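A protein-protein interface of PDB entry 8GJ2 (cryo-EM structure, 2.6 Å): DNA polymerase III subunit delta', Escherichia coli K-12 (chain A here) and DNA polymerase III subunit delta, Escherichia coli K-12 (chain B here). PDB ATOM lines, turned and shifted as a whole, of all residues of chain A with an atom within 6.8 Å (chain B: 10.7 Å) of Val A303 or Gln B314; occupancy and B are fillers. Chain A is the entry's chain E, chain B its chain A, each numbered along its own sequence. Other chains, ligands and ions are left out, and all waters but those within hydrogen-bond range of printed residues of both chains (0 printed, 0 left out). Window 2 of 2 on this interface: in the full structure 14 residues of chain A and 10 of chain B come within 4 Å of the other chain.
The side-chain amino group (NZ) of Lys B313 is in hydrogen-bond range of the backbone carbonyl oxygen (O) of Gly A305 (2.8 Å).
The guanidinium group (NH2) of Arg B248 lies within salt-bridge range of the side-chain carboxylate (OE2) of Glu B309 (2.4 Å).
OE2 of Glu B309 is in salt-bridge range of NZ of Lys B313 (3.6 Å).
Among the printed residues, merely in contact across the chains: Gln A299 with Leu B310 (3.95 Å), Val A303 with Lys B313 (3.98 Å), Val A303 with Gln B314 (3.5 Å), Ile A306 with Glu B309 (3.5 Å), Ile A306 with Leu B310 (3.7 Å), Leu A311 with Thr B306 (3.9 Å) and Leu A311 with Glu B309 (3.7 Å).
Gln A299 touches one residue of chain B.
Of chain B, only Lys B313 (3.98 Å) and Gln B314 (3.5 Å) come within 4 Å of Val A303.
No residue of chain B comes within 4 Å of Thr A304.
Ile A306 touches two residues of chain B.
Of the printed residues of chain A, Thr B306 touches Leu A311.
Of the printed residues of chain A, Glu B309 touches Ile A306 (3.5 Å) and Leu A311 (3.7 Å).
Printed residues of chain A within 4 Å of Leu B310: Gln A299 and Ile A306.
Leu B312 touches none of the printed residues of chain A.
Printed residues of chain A within 4 Å of Lys B313: Val A303 (3.98 Å) and Gly A305 (2.8 Å).
Gln B314 touches one residue of chain A.
Asp B315 touches none of the printed residues of chain A.
The nearest residue of chain B that does not touch Val A303 is Leu B310 (4.8 Å).
The nearest residue of chain A that does not touch Gln B314 is Gln A299 (5.0 Å).
The nearest printed residue of chain B that does not touch Leu A311 is Leu B310 (4.9 Å).
Printed residues of chain A that touch a printed residue of chain B: Gln A299, Val A303, Gly A305, Ile A306 and Leu A311.
Hydrophobic or aromatic side chains of chain A within 4 Å of the printed part of chain B: Val A303, Ile A306 and Leu A311.
Hydrophobic or aromatic side chains of chain B that line the printed part of chain A: Leu B310.
Among the printed residues, 8 pairs touch across the chains.
Among the printed residues, no Asp or Glu carboxylate lies within 4 Å of a Lys or Arg side-chain nitrogen of the other chain.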
ATOM      1  N   GLU A 298      23.501  19.418 -27.582  1.00  0.00           N
ATOM      2  CA  GLU A 298      24.157  19.041 -26.335  1.00  0.00           C
ATOM      3  C   GLU A 298      23.230  18.210 -25.458  1.00  0.00           C
ATOM      4  O   GLU A 298      23.658  17.222 -24.851  1.00  0.00           O
ATOM      5  CB  GLU A 298      24.628  20.291 -25.591  1.00  0.00           C
ATOM      6  CG  GLU A 298      25.367  20.009 -24.289  1.00  0.00           C
ATOM      7  CD  GLU A 298      26.615  19.171 -24.490  1.00  0.00           C
ATOM      8  OE1 GLU A 298      27.121  19.116 -25.631  1.00  0.00           O
ATOM      9  OE2 GLU A 298      27.089  18.564 -23.507  1.00  0.00           O
ATOM     10  N   GLN A 299      21.953  18.594 -25.378  1.00  0.00           N
ATOM     11  CA  GLN A 299      21.003  17.825 -24.580  1.00  0.00           C
ATOM     12  C   GLN A 299      20.837  16.413 -25.129  1.00  0.00           C
ATOM     13  O   GLN A 299      20.788  15.444 -24.363  1.00  0.00           O
ATOM     14  CB  GLN A 299      19.653  18.539 -24.534  1.00  0.00           C
ATOM     15  CG  GLN A 299      19.623  19.743 -23.611  1.00  0.00           C
ATOM     16  CD  GLN A 299      18.254  20.386 -23.539  1.00  0.00           C
ATOM     17  OE1 GLN A 299      17.407  20.164 -24.403  1.00  0.00           O
ATOM     18  NE2 GLN A 299      18.030  21.186 -22.505  1.00  0.00           N
ATOM     19  N   LEU A 300      20.747  16.277 -26.453  1.00  0.00           N
ATOM     20  CA  LEU A 300      20.620  14.950 -27.048  1.00  0.00           C
ATOM     21  C   LEU A 300      21.846  14.098 -26.756  1.00  0.00           C
ATOM     22  O   LEU A 300      21.724  12.908 -26.440  1.00  0.00           O
ATOM     23  CB  LEU A 300      20.401  15.063 -28.557  1.00  0.00           C
ATOM     24  CG  LEU A 300      19.011  15.486 -29.037  1.00  0.00           C
ATOM     25  CD1 LEU A 300      19.016  15.685 -30.543  1.00  0.00           C
ATOM     26  CD2 LEU A 300      17.961  14.462 -28.638  1.00  0.00           C
ATOM     27  N   MET A 301      23.040  14.686 -26.858  1.00  0.00           N
ATOM     28  CA  MET A 301      24.254  13.906 -26.640  1.00  0.00           C
ATOM     29  C   MET A 301      24.464  13.574 -25.167  1.00  0.00           C
ATOM     30  O   MET A 301      25.099  12.563 -24.849  1.00  0.00           O
ATOM     31  CB  MET A 301      25.467  14.660 -27.185  1.00  0.00           C
ATOM     32  CG  MET A 301      25.473  14.810 -28.696  1.00  0.00           C
ATOM     33  SD  MET A 301      26.933  15.665 -29.314  1.00  0.00           S
ATOM     34  CE  MET A 301      28.226  14.508 -28.873  1.00  0.00           C
ATOM     35  N   SER A 302      23.942  14.399 -24.259  1.00  0.00           N
ATOM     36  CA  SER A 302      24.227  14.248 -22.834  1.00  0.00           C
ATOM     37  C   SER A 302      23.176  13.403 -22.117  1.00  0.00           C
ATOM     38  O   SER A 302      23.502  12.373 -21.517  1.00  0.00           O
ATOM     39  CB  SER A 302      24.332  15.630 -22.179  1.00  0.00           C
ATOM     40  OG  SER A 302      24.581  15.516 -20.789  1.00  0.00           O
ATOM     41  N   VAL A 303      21.912  13.828 -22.167  1.00  0.00           N
ATOM     42  CA  VAL A 303      20.871  13.150 -21.403  1.00  0.00           C
ATOM     43  C   VAL A 303      20.678  11.735 -21.930  1.00  0.00           C
ATOM     44  O   VAL A 303      20.678  11.493 -23.145  1.00  0.00           O
ATOM     45  CB  VAL A 303      19.556  13.947 -21.459  1.00  0.00           C
ATOM     46  CG1 VAL A 303      18.476  13.248 -20.645  1.00  0.00           C
ATOM     47  CG2 VAL A 303      19.773  15.367 -20.955  1.00  0.00           C
ATOM     48  N   THR A 304      20.509  10.790 -21.009  1.00  0.00           N
ATOM     49  CA  THR A 304      20.322   9.384 -21.343  1.00  0.00           C
ATOM     50  C   THR A 304      18.837   9.050 -21.335  1.00  0.00           C
ATOM     51  O   THR A 304      18.128   9.371 -20.376  1.00  0.00           O
ATOM     52  CB  THR A 304      21.066   8.485 -20.353  1.00  0.00           C
ATOM     53  OG1 THR A 304      20.552   8.696 -19.031  1.00  0.00           O
ATOM     54  CG2 THR A 304      22.557   8.787 -20.368  1.00  0.00           C
ATOM     55  N   GLY A 305      18.374   8.402 -22.402  1.00  0.00           N
ATOM     56  CA  GLY A 305      16.982   8.027 -22.525  1.00  0.00           C
ATOM     57  C   GLY A 305      16.064   9.118 -23.028  1.00  0.00           C
ATOM     58  O   GLY A 305      14.846   8.904 -23.075  1.00  0.00           O
ATOM     59  N   ILE A 306      16.601  10.279 -23.406  1.00  0.00           N
ATOM     60  CA  ILE A 306      15.761  11.369 -23.886  1.00  0.00           C
ATOM     61  C   ILE A 306      15.120  10.974 -25.212  1.00  0.00           C
ATOM     62  O   ILE A 306      15.696  10.228 -26.014  1.00  0.00           O
ATOM     63  CB  ILE A 306      16.591  12.660 -24.025  1.00  0.00           C
ATOM     64  CG1 ILE A 306      15.683  13.879 -24.210  1.00  0.00           C
ATOM     65  CG2 ILE A 306      17.559  12.548 -25.194  1.00  0.00           C
ATOM     66  CD1 ILE A 306      14.838  14.210 -22.998  1.00  0.00           C
ATOM     67  N   LEU A 311      11.977  16.280 -28.709  1.00  0.00           N
ATOM     68  CA  LEU A 311      12.905  17.403 -28.643  1.00  0.00           C
ATOM     69  C   LEU A 311      13.016  18.111 -29.987  1.00  0.00           C
ATOM     70  O   LEU A 311      13.005  19.346 -30.046  1.00  0.00           O
ATOM     71  CB  LEU A 311      14.281  16.926 -28.179  1.00  0.00           C
ATOM     72  CG  LEU A 311      14.566  17.081 -26.683  1.00  0.00           C
ATOM     73  CD1 LEU A 311      13.577  16.279 -25.852  1.00  0.00           C
ATOM     74  CD2 LEU A 311      15.994  16.667 -26.370  1.00  0.00           C
ATOM     75  N   LEU B 247       3.509   9.786 -20.003  1.00  0.00           N
ATOM     76  CA  LEU B 247       4.119  10.775 -20.883  1.00  0.00           C
ATOM     77  C   LEU B 247       4.143  10.281 -22.324  1.00  0.00           C
ATOM     78  O   LEU B 247       3.797  11.020 -23.248  1.00  0.00           O
ATOM     79  CB  LEU B 247       5.534  11.103 -20.404  1.00  0.00           C
ATOM     80  CG  LEU B 247       5.658  11.823 -19.058  1.00  0.00           C
ATOM     81  CD1 LEU B 247       7.118  11.948 -18.659  1.00  0.00           C
ATOM     82  CD2 LEU B 247       5.003  13.192 -19.105  1.00  0.00           C
ATOM     83  N   ARG B 248       4.537   9.023 -22.533  1.00  0.00           N
ATOM     84  CA  ARG B 248       4.595   8.487 -23.892  1.00  0.00           C
ATOM     85  C   ARG B 248       3.203   8.361 -24.505  1.00  0.00           C
ATOM     86  O   ARG B 248       2.999   8.693 -25.686  1.00  0.00           O
ATOM     87  CB  ARG B 248       5.302   7.132 -23.888  1.00  0.00           C
ATOM     88  CG  ARG B 248       6.764   7.203 -23.483  1.00  0.00           C
ATOM     89  CD  ARG B 248       7.630   7.766 -24.598  1.00  0.00           C
ATOM     90  NE  ARG B 248       8.842   8.390 -24.081  1.00  0.00           N
ATOM     91  CZ  ARG B 248       8.933   9.655 -23.691  1.00  0.00           C
ATOM     92  NH1 ARG B 248       7.898  10.477 -23.748  1.00  0.00           N
ATOM     93  NH2 ARG B 248      10.095  10.106 -23.230  1.00  0.00           N
ATOM     94  N   THR B 306       7.789  18.621 -23.008  1.00  0.00           N
ATOM     95  CA  THR B 306       9.238  18.489 -23.133  1.00  0.00           C
ATOM     96  C   THR B 306       9.939  18.904 -21.846  1.00  0.00           C
ATOM     97  O   THR B 306      10.894  18.251 -21.409  1.00  0.00           O
ATOM     98  CB  THR B 306       9.743  19.325 -24.308  1.00  0.00           C
ATOM     99  OG1 THR B 306       9.046  18.948 -25.501  1.00  0.00           O
ATOM    100  CG2 THR B 306      11.236  19.117 -24.513  1.00  0.00           C
ATOM    101  N   ARG B 307       9.483  19.996 -21.228  1.00  0.00           N
ATOM    102  CA  ARG B 307      10.079  20.432 -19.970  1.00  0.00           C
ATOM    103  C   ARG B 307       9.891  19.380 -18.885  1.00  0.00           C
ATOM    104  O   ARG B 307      10.814  19.099 -18.111  1.00  0.00           O
ATOM    105  CB  ARG B 307       9.466  21.764 -19.539  1.00  0.00           C
ATOM    106  CG  ARG B 307      10.327  22.565 -18.581  1.00  0.00           C
ATOM    107  CD  ARG B 307       9.554  23.737 -18.005  1.00  0.00           C
ATOM    108  NE  ARG B 307       8.587  23.307 -17.002  1.00  0.00           N
ATOM    109  CZ  ARG B 307       7.610  24.066 -16.523  1.00  0.00           C
ATOM    110  NH1 ARG B 307       7.417  25.301 -16.955  1.00  0.00           N
ATOM    111  NH2 ARG B 307       6.804  23.570 -15.589  1.00  0.00           N
ATOM    112  N   THR B 308       8.697  18.788 -18.813  1.00  0.00           N
ATOM    113  CA  THR B 308       8.444  17.738 -17.832  1.00  0.00           C
ATOM    114  C   THR B 308       9.343  16.535 -18.076  1.00  0.00           C
ATOM    115  O   THR B 308       9.882  15.952 -17.128  1.00  0.00           O
ATOM    116  CB  THR B 308       6.974  17.319 -17.882  1.00  0.00           C
ATOM    117  OG1 THR B 308       6.138  18.479 -17.778  1.00  0.00           O
ATOM    118  CG2 THR B 308       6.649  16.364 -16.746  1.00  0.00           C
ATOM    119  N   GLU B 309       9.511  16.143 -19.340  1.00  0.00           N
ATOM    120  CA  GLU B 309      10.384  15.015 -19.647  1.00  0.00           C
ATOM    121  C   GLU B 309      11.818  15.307 -19.228  1.00  0.00           C
ATOM    122  O   GLU B 309      12.484  14.452 -18.634  1.00  0.00           O
ATOM    123  CB  GLU B 309      10.325  14.690 -21.138  1.00  0.00           C
ATOM    124  CG  GLU B 309      11.023  13.386 -21.510  1.00  0.00           C
ATOM    125  CD  GLU B 309      11.288  13.259 -22.997  1.00  0.00           C
ATOM    126  OE1 GLU B 309      11.378  14.300 -23.681  1.00  0.00           O
ATOM    127  OE2 GLU B 309      11.407  12.115 -23.482  1.00  0.00           O
ATOM    128  N   LEU B 310      12.315  16.507 -19.533  1.00  0.00           N
ATOM    129  CA  LEU B 310      13.678  16.852 -19.143  1.00  0.00           C
ATOM    130  C   LEU B 310      13.833  16.836 -17.628  1.00  0.00           C
ATOM    131  O   LEU B 310      14.816  16.301 -17.101  1.00  0.00           O
ATOM    132  CB  LEU B 310      14.059  18.221 -19.707  1.00  0.00           C
ATOM    133  CG  LEU B 310      14.322  18.284 -21.212  1.00  0.00           C
ATOM    134  CD1 LEU B 310      14.456  19.727 -21.666  1.00  0.00           C
ATOM    135  CD2 LEU B 310      15.570  17.494 -21.578  1.00  0.00           C
ATOM    136  N   THR B 311      12.861  17.404 -16.908  1.00  0.00           N
ATOM    137  CA  THR B 311      12.932  17.410 -15.452  1.00  0.00           C
ATOM    138  C   THR B 311      12.943  15.992 -14.898  1.00  0.00           C
ATOM    139  O   THR B 311      13.701  15.684 -13.973  1.00  0.00           O
ATOM    140  CB  THR B 311      11.758  18.199 -14.872  1.00  0.00           C
ATOM    141  OG1 THR B 311      11.798  19.548 -15.357  1.00  0.00           O
ATOM    142  CG2 THR B 311      11.816  18.209 -13.351  1.00  0.00           C
ATOM    143  N   LEU B 312      12.105  15.113 -15.451  1.00  0.00           N
ATOM    144  CA  LEU B 312      12.072  13.733 -14.983  1.00  0.00           C
ATOM    145  C   LEU B 312      13.390  13.022 -15.267  1.00  0.00           C
ATOM    146  O   LEU B 312      13.886  12.262 -14.426  1.00  0.00           O
ATOM    147  CB  LEU B 312      10.910  12.987 -15.639  1.00  0.00           C
ATOM    148  CG  LEU B 312      10.764  11.504 -15.290  1.00  0.00           C
ATOM    149  CD1 LEU B 312      10.573  11.313 -13.793  1.00  0.00           C
ATOM    150  CD2 LEU B 312       9.606  10.892 -16.059  1.00  0.00           C
ATOM    151  N   LYS B 313      13.974  13.256 -16.442  1.00  0.00           N
ATOM    152  CA  LYS B 313      15.143  12.484 -16.854  1.00  0.00           C
ATOM    153  C   LYS B 313      16.418  12.982 -16.180  1.00  0.00           C
ATOM    154  O   LYS B 313      17.081  12.230 -15.459  1.00  0.00           O
ATOM    155  CB  LYS B 313      15.289  12.526 -18.379  1.00  0.00           C
ATOM    156  CG  LYS B 313      14.133  11.889 -19.140  1.00  0.00           C
ATOM    157  CD  LYS B 313      14.078  10.382 -18.964  1.00  0.00           C
ATOM    158  CE  LYS B 313      12.877   9.794 -19.687  1.00  0.00           C
ATOM    159  NZ  LYS B 313      12.991   9.918 -21.165  1.00  0.00           N
ATOM    160  N   GLN B 314      16.781  14.247 -16.401  1.00  0.00           N
ATOM    161  CA  GLN B 314      18.077  14.726 -15.927  1.00  0.00           C
ATOM    162  C   GLN B 314      18.033  15.278 -14.509  1.00  0.00           C
ATOM    163  O   GLN B 314      18.980  15.064 -13.745  1.00  0.00           O
ATOM    164  CB  GLN B 314      18.631  15.796 -16.878  1.00  0.00           C
ATOM    165  CG  GLN B 314      17.993  17.174 -16.762  1.00  0.00           C
ATOM    166  CD  GLN B 314      18.536  18.149 -17.786  1.00  0.00           C
ATOM    167  OE1 GLN B 314      19.446  17.824 -18.546  1.00  0.00           O
ATOM    168  NE2 GLN B 314      17.979  19.354 -17.809  1.00  0.00           N
ATOM    169  N   ASP B 315      16.964  15.982 -14.133  1.00  0.00           N
ATOM    170  CA  ASP B 315      16.893  16.598 -12.815  1.00  0.00           C
ATOM    171  C   ASP B 315      16.392  15.654 -11.732  1.00  0.00           C
ATOM    172  O   ASP B 315      16.600  15.933 -10.546  1.00  0.00           O
ATOM    173  CB  ASP B 315      15.988  17.833 -12.859  1.00  0.00           C
ATOM    174  CG  ASP B 315      16.521  18.916 -13.774  1.00  0.00           C
ATOM    175  OD1 ASP B 315      17.758  19.040 -13.893  1.00  0.00           O
ATOM    176  OD2 ASP B 315      15.704  19.645 -14.376  1.00  0.00           O
ATOM    177  N   TYR B 316      15.751  14.548 -12.105  1.00  0.00           N
ATOM    178  CA  TYR B 316      15.202  13.600 -11.135  1.00  0.00           C
ATOM    179  C   TYR B 316      14.265  14.304 -10.155  1.00  0.00           C
ATOM    180  O   TYR B 316      14.263  14.027  -8.954  1.00  0.00           O
ATOM    181  CB  TYR B 316      16.320  12.874 -10.386  1.00  0.00           C
ATOM    182  CG  TYR B 316      17.359  12.252 -11.291  1.00  0.00           C
ATOM    183  CD1 TYR B 316      17.073  11.113 -12.028  1.00  0.00           C
ATOM    184  CD2 TYR B 316      18.627  12.803 -11.403  1.00  0.00           C
ATOM    185  CE1 TYR B 316      18.019  10.542 -12.856  1.00  0.00           C
ATOM    186  CE2 TYR B 316      19.580  12.239 -12.228  1.00  0.00           C
ATOM    187  CZ  TYR B 316      19.270  11.109 -12.952  1.00  0.00           C
ATOM    188  OH  TYR B 316      20.218  10.545 -13.774  1.00  0.00           O
ATOM    189  N   GLY B 317      13.461  15.223 -10.676  1.00  0.00           N
ATOM    190  CA  GLY B 317      12.550  15.975  -9.841  1.00  0.00           C
ATOM    191  C   GLY B 317      11.361  15.148  -9.391  1.00  0.00           C
ATOM    192  O   GLY B 317      11.054  14.082  -9.927  1.00  0.00           O
ATOM    193  N   GLN B 318      10.676  15.665  -8.370  1.00  0.00           N
ATOM    194  CA  GLN B 318       9.512  15.009  -7.791  1.00  0.00           C
ATOM    195  C   GLN B 318       8.207  15.729  -8.102  1.00  0.00           C
ATOM    196  O   GLN B 318       7.151  15.291  -7.635  1.00  0.00           O
ATOM    197  CB  GLN B 318       9.679  14.892  -6.270  1.00  0.00           C
ATOM    198  CG  GLN B 318      10.998  14.275  -5.829  1.00  0.00           C
ATOM    199  CD  GLN B 318      11.195  12.869  -6.362  1.00  0.00           C
ATOM    200  OE1 GLN B 318      10.239  12.205  -6.763  1.00  0.00           O
ATOM    201  NE2 GLN B 318      12.440  12.409  -6.371  1.00  0.00           N
